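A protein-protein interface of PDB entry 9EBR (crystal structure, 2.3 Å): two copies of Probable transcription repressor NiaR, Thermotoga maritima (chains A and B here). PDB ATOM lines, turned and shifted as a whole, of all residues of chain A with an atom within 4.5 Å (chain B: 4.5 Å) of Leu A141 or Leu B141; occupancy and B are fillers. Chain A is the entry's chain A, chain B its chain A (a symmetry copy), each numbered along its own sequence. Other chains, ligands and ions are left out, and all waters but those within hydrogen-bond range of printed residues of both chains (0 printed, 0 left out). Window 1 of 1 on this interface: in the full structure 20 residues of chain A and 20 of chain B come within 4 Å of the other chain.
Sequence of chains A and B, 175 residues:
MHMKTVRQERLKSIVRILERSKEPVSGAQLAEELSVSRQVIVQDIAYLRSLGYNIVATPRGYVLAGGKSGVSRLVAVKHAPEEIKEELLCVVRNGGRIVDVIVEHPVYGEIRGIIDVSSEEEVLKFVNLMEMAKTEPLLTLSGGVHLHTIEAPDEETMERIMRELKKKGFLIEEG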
ATOM      1  N   VAL A 103      31.225  -2.886   3.298  1.00  0.00           N
ATOM      2  CA  VAL A 103      30.246  -1.844   3.531  1.00  0.00           C
ATOM      3  C   VAL A 103      29.338  -2.256   4.679  1.00  0.00           C
ATOM      4  O   VAL A 103      28.971  -3.431   4.814  1.00  0.00           O
ATOM      5  CB  VAL A 103      29.461  -1.582   2.243  1.00  0.00           C
ATOM      6  CG1 VAL A 103      28.181  -0.841   2.554  1.00  0.00           C
ATOM      7  CG2 VAL A 103      30.337  -0.790   1.306  1.00  0.00           C
ATOM      8  N   HIS A 105      25.935  -2.117   5.714  1.00  0.00           N
ATOM      9  CA  HIS A 105      24.648  -1.799   5.112  1.00  0.00           C
ATOM     10  C   HIS A 105      23.581  -1.689   6.200  1.00  0.00           C
ATOM     11  O   HIS A 105      23.426  -2.618   7.007  1.00  0.00           O
ATOM     12  CB  HIS A 105      24.273  -2.861   4.086  1.00  0.00           C
ATOM     13  CG  HIS A 105      23.046  -2.538   3.290  1.00  0.00           C
ATOM     14  ND1 HIS A 105      21.777  -2.579   3.830  1.00  0.00           N
ATOM     15  CD2 HIS A 105      22.893  -2.178   1.993  1.00  0.00           C
ATOM     16  CE1 HIS A 105      20.897  -2.264   2.894  1.00  0.00           C
ATOM     17  NE2 HIS A 105      21.550  -2.000   1.779  1.00  0.00           N
ATOM     18  N   LYS A 134      26.397  -1.766 -15.804  1.00  0.00           N
ATOM     19  CA  LYS A 134      25.658  -2.551 -14.819  1.00  0.00           C
ATOM     20  C   LYS A 134      26.596  -3.213 -13.809  1.00  0.00           C
ATOM     21  O   LYS A 134      26.311  -4.294 -13.285  1.00  0.00           O
ATOM     22  CB  LYS A 134      24.755  -3.589 -15.503  1.00  0.00           C
ATOM     23  CG  LYS A 134      23.629  -2.973 -16.340  1.00  0.00           C
ATOM     24  CD  LYS A 134      22.912  -1.856 -15.569  1.00  0.00           C
ATOM     25  CE  LYS A 134      22.601  -0.651 -16.461  1.00  0.00           C
ATOM     26  NZ  LYS A 134      22.047   0.523 -15.713  1.00  0.00           N
ATOM     27  N   THR A 135      27.726  -2.566 -13.539  1.00  0.00           N
ATOM     28  CA  THR A 135      28.604  -2.960 -12.447  1.00  0.00           C
ATOM     29  C   THR A 135      28.913  -1.708 -11.636  1.00  0.00           C
ATOM     30  O   THR A 135      29.424  -0.721 -12.178  1.00  0.00           O
ATOM     31  CB  THR A 135      29.880  -3.637 -12.966  1.00  0.00           C
ATOM     32  OG1 THR A 135      30.931  -2.679 -13.081  1.00  0.00           O
ATOM     33  CG2 THR A 135      29.642  -4.296 -14.342  1.00  0.00           C
ATOM     34  N   GLU A 136      28.572  -1.741 -10.350  1.00  0.00           N
ATOM     35  CA  GLU A 136      28.673  -0.616  -9.433  1.00  0.00           C
ATOM     36  C   GLU A 136      29.422  -1.023  -8.176  1.00  0.00           C
ATOM     37  O   GLU A 136      29.211  -2.127  -7.664  1.00  0.00           O
ATOM     38  CB  GLU A 136      27.280  -0.124  -9.051  1.00  0.00           C
ATOM     39  CG  GLU A 136      26.429   0.108 -10.252  1.00  0.00           C
ATOM     40  CD  GLU A 136      26.912   1.302 -11.039  1.00  0.00           C
ATOM     41  OE1 GLU A 136      27.399   2.254 -10.391  1.00  0.00           O
ATOM     42  OE2 GLU A 136      26.820   1.275 -12.288  1.00  0.00           O
ATOM     43  N   PRO A 137      30.275  -0.161  -7.635  1.00  0.00           N
ATOM     44  CA  PRO A 137      31.046  -0.533  -6.444  1.00  0.00           C
ATOM     45  C   PRO A 137      30.162  -0.591  -5.206  1.00  0.00           C
ATOM     46  O   PRO A 137      29.103   0.033  -5.135  1.00  0.00           O
ATOM     47  CB  PRO A 137      32.091   0.582  -6.326  1.00  0.00           C
ATOM     48  CG  PRO A 137      31.982   1.381  -7.617  1.00  0.00           C
ATOM     49  CD  PRO A 137      30.599   1.190  -8.114  1.00  0.00           C
ATOM     50  N   LEU A 138      30.620  -1.349  -4.206  1.00  0.00           N
ATOM     51  CA  LEU A 138      29.813  -1.498  -2.999  1.00  0.00           C
ATOM     52  C   LEU A 138      29.540  -0.151  -2.333  1.00  0.00           C
ATOM     53  O   LEU A 138      28.447   0.055  -1.793  1.00  0.00           O
ATOM     54  CB  LEU A 138      30.488  -2.476  -2.028  1.00  0.00           C
ATOM     55  CG  LEU A 138      30.597  -3.904  -2.570  1.00  0.00           C
ATOM     56  CD1 LEU A 138      31.089  -4.933  -1.558  1.00  0.00           C
ATOM     57  CD2 LEU A 138      29.252  -4.324  -3.128  1.00  0.00           C
ATOM     58  N   LEU A 139      30.493   0.790  -2.378  1.00  0.00           N
ATOM     59  CA  LEU A 139      30.287   2.076  -1.710  1.00  0.00           C
ATOM     60  C   LEU A 139      29.010   2.778  -2.161  1.00  0.00           C
ATOM     61  O   LEU A 139      28.567   3.720  -1.483  1.00  0.00           O
ATOM     62  CB  LEU A 139      31.507   2.991  -1.921  1.00  0.00           C
ATOM     63  CG  LEU A 139      31.907   3.341  -3.359  1.00  0.00           C
ATOM     64  CD1 LEU A 139      31.169   4.570  -3.842  1.00  0.00           C
ATOM     65  CD2 LEU A 139      33.420   3.501  -3.509  1.00  0.00           C
ATOM     66  N   THR A 140      28.391   2.338  -3.263  1.00  0.00           N
ATOM     67  CA  THR A 140      27.159   2.978  -3.707  1.00  0.00           C
ATOM     68  C   THR A 140      25.970   2.579  -2.842  1.00  0.00           C
ATOM     69  O   THR A 140      24.951   3.277  -2.836  1.00  0.00           O
ATOM     70  CB  THR A 140      26.895   2.657  -5.177  1.00  0.00           C
ATOM     71  OG1 THR A 140      26.958   1.242  -5.391  1.00  0.00           O
ATOM     72  CG2 THR A 140      27.929   3.320  -6.052  1.00  0.00           C
ATOM     73  N   LEU A 141      26.085   1.473  -2.106  1.00  0.00           N
ATOM     74  CA  LEU A 141      25.063   1.108  -1.135  1.00  0.00           C
ATOM     75  C   LEU A 141      25.176   1.947   0.116  1.00  0.00           C
ATOM     76  O   LEU A 141      24.193   2.114   0.853  1.00  0.00           O
ATOM     77  CB  LEU A 141      25.219  -0.360  -0.760  1.00  0.00           C
ATOM     78  CG  LEU A 141      24.977  -1.298  -1.924  1.00  0.00           C
ATOM     79  CD1 LEU A 141      25.443  -2.672  -1.567  1.00  0.00           C
ATOM     80  CD2 LEU A 141      23.485  -1.285  -2.171  1.00  0.00           C
ATOM     81  N   SER A 142      26.368   2.494   0.346  1.00  0.00           N
ATOM     82  CA  SER A 142      26.809   2.979   1.641  1.00  0.00           C
ATOM     83  C   SER A 142      26.973   4.486   1.660  1.00  0.00           C
ATOM     84  O   SER A 142      27.609   5.027   2.574  1.00  0.00           O
ATOM     85  CB  SER A 142      28.126   2.284   2.003  1.00  0.00           C
ATOM     86  OG  SER A 142      28.358   2.317   3.403  1.00  0.00           O
ATOM     87  N   GLY A 143      26.430   5.179   0.662  1.00  0.00           N
ATOM     88  CA  GLY A 143      26.637   6.614   0.576  1.00  0.00           C
ATOM     89  C   GLY A 143      28.092   7.015   0.542  1.00  0.00           C
ATOM     90  O   GLY A 143      28.426   8.140   0.922  1.00  0.00           O
ATOM     91  N   VAL B 103      22.873 -11.239  -5.345  1.00  0.00           N
ATOM     92  CA  VAL B 103      23.224 -10.600  -6.596  1.00  0.00           C
ATOM     93  C   VAL B 103      24.513 -11.209  -7.126  1.00  0.00           C
ATOM     94  O   VAL B 103      25.434 -11.521  -6.359  1.00  0.00           O
ATOM     95  CB  VAL B 103      23.348  -9.089  -6.383  1.00  0.00           C
ATOM     96  CG1 VAL B 103      24.118  -8.463  -7.523  1.00  0.00           C
ATOM     97  CG2 VAL B 103      21.961  -8.510  -6.277  1.00  0.00           C
ATOM     98  N   HIS B 105      27.529 -10.311  -8.789  1.00  0.00           N
ATOM     99  CA  HIS B 105      28.240  -9.085  -9.124  1.00  0.00           C
ATOM    100  C   HIS B 105      29.383  -9.397 -10.088  1.00  0.00           C
ATOM    101  O   HIS B 105      30.210 -10.274  -9.801  1.00  0.00           O
ATOM    102  CB  HIS B 105      28.765  -8.422  -7.856  1.00  0.00           C
ATOM    103  CG  HIS B 105      29.365  -7.067  -8.075  1.00  0.00           C
ATOM    104  ND1 HIS B 105      30.583  -6.887  -8.700  1.00  0.00           N
ATOM    105  CD2 HIS B 105      28.923  -5.830  -7.746  1.00  0.00           C
ATOM    106  CE1 HIS B 105      30.863  -5.595  -8.737  1.00  0.00           C
ATOM    107  NE2 HIS B 105      29.865  -4.936  -8.182  1.00  0.00           N
ATOM    108  N   LYS B 134      20.521   6.889   2.093  1.00  0.00           N
ATOM    109  CA  LYS B 134      21.808   6.204   1.999  1.00  0.00           C
ATOM    110  C   LYS B 134      21.674   4.711   2.295  1.00  0.00           C
ATOM    111  O   LYS B 134      22.599   4.076   2.811  1.00  0.00           O
ATOM    112  CB  LYS B 134      22.854   6.861   2.913  1.00  0.00           C
ATOM    113  CG  LYS B 134      23.214   8.294   2.509  1.00  0.00           C
ATOM    114  CD  LYS B 134      23.478   8.395   0.999  1.00  0.00           C
ATOM    115  CE  LYS B 134      22.866   9.661   0.394  1.00  0.00           C
ATOM    116  NZ  LYS B 134      22.961   9.719  -1.100  1.00  0.00           N
ATOM    117  N   THR B 135      20.513   4.146   1.974  1.00  0.00           N
ATOM    118  CA  THR B 135      20.320   2.704   1.995  1.00  0.00           C
ATOM    119  C   THR B 135      19.691   2.308   0.666  1.00  0.00           C
ATOM    120  O   THR B 135      18.623   2.814   0.303  1.00  0.00           O
ATOM    121  CB  THR B 135      19.460   2.267   3.191  1.00  0.00           C
ATOM    122  OG1 THR B 135      18.094   2.153   2.793  1.00  0.00           O
ATOM    123  CG2 THR B 135      19.567   3.276   4.353  1.00  0.00           C
ATOM    124  N   GLU B 136      20.372   1.431  -0.070  1.00  0.00           N
ATOM    125  CA  GLU B 136      20.009   1.012  -1.414  1.00  0.00           C
ATOM    126  C   GLU B 136      19.977  -0.504  -1.505  1.00  0.00           C
ATOM    127  O   GLU B 136      20.848  -1.173  -0.942  1.00  0.00           O
ATOM    128  CB  GLU B 136      21.015   1.556  -2.423  1.00  0.00           C
ATOM    129  CG  GLU B 136      21.233   3.019  -2.250  1.00  0.00           C
ATOM    130  CD  GLU B 136      20.013   3.804  -2.664  1.00  0.00           C
ATOM    131  OE1 GLU B 136      19.338   3.354  -3.614  1.00  0.00           O
ATOM    132  OE2 GLU B 136      19.725   4.847  -2.028  1.00  0.00           O
ATOM    133  N   PRO B 137      19.015  -1.079  -2.220  1.00  0.00           N
ATOM    134  CA  PRO B 137      18.930  -2.541  -2.300  1.00  0.00           C
ATOM    135  C   PRO B 137      20.051  -3.118  -3.153  1.00  0.00           C
ATOM    136  O   PRO B 137      20.626  -2.448  -4.009  1.00  0.00           O
ATOM    137  CB  PRO B 137      17.561  -2.788  -2.944  1.00  0.00           C
ATOM    138  CG  PRO B 137      16.867  -1.433  -2.959  1.00  0.00           C
ATOM    139  CD  PRO B 137      17.939  -0.412  -2.965  1.00  0.00           C
ATOM    140  N   LEU B 138      20.353  -4.399  -2.918  1.00  0.00           N
ATOM    141  CA  LEU B 138      21.446  -5.018  -3.658  1.00  0.00           C
ATOM    142  C   LEU B 138      21.203  -4.979  -5.166  1.00  0.00           C
ATOM    143  O   LEU B 138      22.153  -4.804  -5.937  1.00  0.00           O
ATOM    144  CB  LEU B 138      21.672  -6.455  -3.167  1.00  0.00           C
ATOM    145  CG  LEU B 138      22.127  -6.540  -1.707  1.00  0.00           C
ATOM    146  CD1 LEU B 138      22.539  -7.935  -1.251  1.00  0.00           C
ATOM    147  CD2 LEU B 138      23.264  -5.563  -1.488  1.00  0.00           C
ATOM    148  N   LEU B 139      19.946  -5.105  -5.614  1.00  0.00           N
ATOM    149  CA  LEU B 139      19.676  -5.119  -7.052  1.00  0.00           C
ATOM    150  C   LEU B 139      20.235  -3.894  -7.770  1.00  0.00           C
ATOM    151  O   LEU B 139      20.333  -3.912  -9.008  1.00  0.00           O
ATOM    152  CB  LEU B 139      18.165  -5.253  -7.315  1.00  0.00           C
ATOM    153  CG  LEU B 139      17.235  -4.179  -6.740  1.00  0.00           C
ATOM    154  CD1 LEU B 139      17.082  -3.024  -7.702  1.00  0.00           C
ATOM    155  CD2 LEU B 139      15.877  -4.756  -6.337  1.00  0.00           C
ATOM    156  N   THR B 140      20.627  -2.845  -7.036  1.00  0.00           N
ATOM    157  CA  THR B 140      21.182  -1.668  -7.694  1.00  0.00           C
ATOM    158  C   THR B 140      22.608  -1.906  -8.173  1.00  0.00           C
ATOM    159  O   THR B 140      23.094  -1.177  -9.044  1.00  0.00           O
ATOM    160  CB  THR B 140      21.114  -0.459  -6.762  1.00  0.00           C
ATOM    161  OG1 THR B 140      21.699  -0.782  -5.494  1.00  0.00           O
ATOM    162  CG2 THR B 140      19.681  -0.050  -6.536  1.00  0.00           C
ATOM    163  N   LEU B 141      23.282  -2.917  -7.627  1.00  0.00           N
ATOM    164  CA  LEU B 141      24.588  -3.312  -8.136  1.00  0.00           C
ATOM    165  C   LEU B 141      24.455  -4.099  -9.418  1.00  0.00           C
ATOM    166  O   LEU B 141      25.396  -4.151 -10.225  1.00  0.00           O
ATOM    167  CB  LEU B 141      25.301  -4.172  -7.100  1.00  0.00           C
ATOM    168  CG  LEU B 141      25.612  -3.423  -5.822  1.00  0.00           C
ATOM    169  CD1 LEU B 141      26.020  -4.391  -4.759  1.00  0.00           C
ATOM    170  CD2 LEU B 141      26.748  -2.481  -6.152  1.00  0.00           C
ATOM    171  N   SER B 142      23.281  -4.697  -9.619  1.00  0.00           N
ATOM    172  CA  SER B 142      23.071  -5.797 -10.540  1.00  0.00           C
ATOM    173  C   SER B 142      22.195  -5.400 -11.714  1.00  0.00           C
ATOM    174  O   SER B 142      21.684  -6.273 -12.426  1.00  0.00           O
ATOM    175  CB  SER B 142      22.450  -6.969  -9.771  1.00  0.00           C
ATOM    176  OG  SER B 142      22.664  -8.199 -10.445  1.00  0.00           O
ATOM    177  N   GLY B 143      21.997  -4.100 -11.922  1.00  0.00           N
ATOM    178  CA  GLY B 143      21.091  -3.663 -12.971  1.00  0.00           C
ATOM    179  C   GLY B 143      19.696  -4.225 -12.839  1.00  0.00           C
ATOM    180  O   GLY B 143      18.980  -4.328 -13.840  1.00  0.00           O
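NE2 of His A105 is in hydrogen-bond range of O of Glu B136.
The backbone carbonyl oxygen (O) of Glu A136 is in hydrogen-bond range of a ring nitrogen (NE2) of His B105 (2.9 Å).
The backbone carbonyl oxygen (O) of Leu B141 lies close to the backbone carbonyl oxygen (O) of Lys A134, at 3.2 Å.
O of Leu A141 lies close to O of Lys B134.
O of Pro A137 lies within hydrogen-bond range of OG1 of Thr A140 (2.5 Å).
The side-chain hydroxyl of Thr B140 sits at hydrogen-bond distance from the backbone carbonyl oxygen of Pro B137.
Among the printed residues, pairs that only touch across the chains: Lys A134 with Gly B143 (3.7 Å), Glu A136 with Thr B140 (3.8 Å), Glu A136 with Leu B141 (2.9 Å), Pro A137 with Leu B141 (3.6 Å), Leu A138 with Leu B141 (3.6 Å), Thr A140 with Glu B136 (3.8 Å), Thr A140 with Leu B141 (3.8 Å), Leu A141 with Glu B136 (2.9 Å), Leu A141 with Pro B137 (3.6 Å), Leu A141 with Leu B138 (3.6 Å), Leu A141 with Thr B140 (3.8 Å), Leu A141 with Leu B141 (3.7 Å) and Gly A143 with Lys B134 (3.7 Å).
Thr A135 touches none of the printed residues of chain B.
Of the printed residues of chain B, Leu A138 touches Leu B141.
Of the printed residues of chain B, Thr A140 touches Glu B136 (3.8 Å) and Leu B141 (3.8 Å).
Leu A141 touches six residues of chain B.
Of the printed residues of chain B, Gly A143 touches Lys B134.
Of the printed residues of chain A, Leu B138 touches Leu A141.
Leu B139 touches none of the printed residues of chain A.
Of the printed residues of chain A, Thr B140 touches Glu A136 (3.8 Å) and Leu A141 (3.8 Å).
Leu B141 touches just these residues of chain A: Lys A134 (3.2 Å), Glu A136 (2.9 Å), Pro A137 (3.6 Å), Leu A138 (3.6 Å), Thr A140 (3.8 Å) and Leu A141 (3.7 Å).
The nearest residue of chain A that does not touch Leu B141 is Thr A135 (4.1 Å).
Printed residues of chain B that touch a printed residue of chain A: His B105, Lys B134, Glu B136, Pro B137, Leu B138, Thr B140, Leu B141 and Gly B143.
Hydrophobic or aromatic side chains of chain B that line the printed part of chain A: His B105, Leu B138 and Leu B141.
Hydrophobic or aromatic side chains of chain A within 4 Å of the printed part of chain B: His A105, Leu A138 and Leu A141.
Among the printed residues, 17 pairs touch across the chains.
His A105 touches Glu B136, and with the chains exchanged Glu A136 touches His B105.
Glu A136 touches Thr B140, and with the chains exchanged Thr A140 touches Glu B136.
Leu A138 touches Leu B141, and with the chains exchanged Leu A141 touches Leu B138.
Leu B141 touches its own counterpart, Leu A141.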
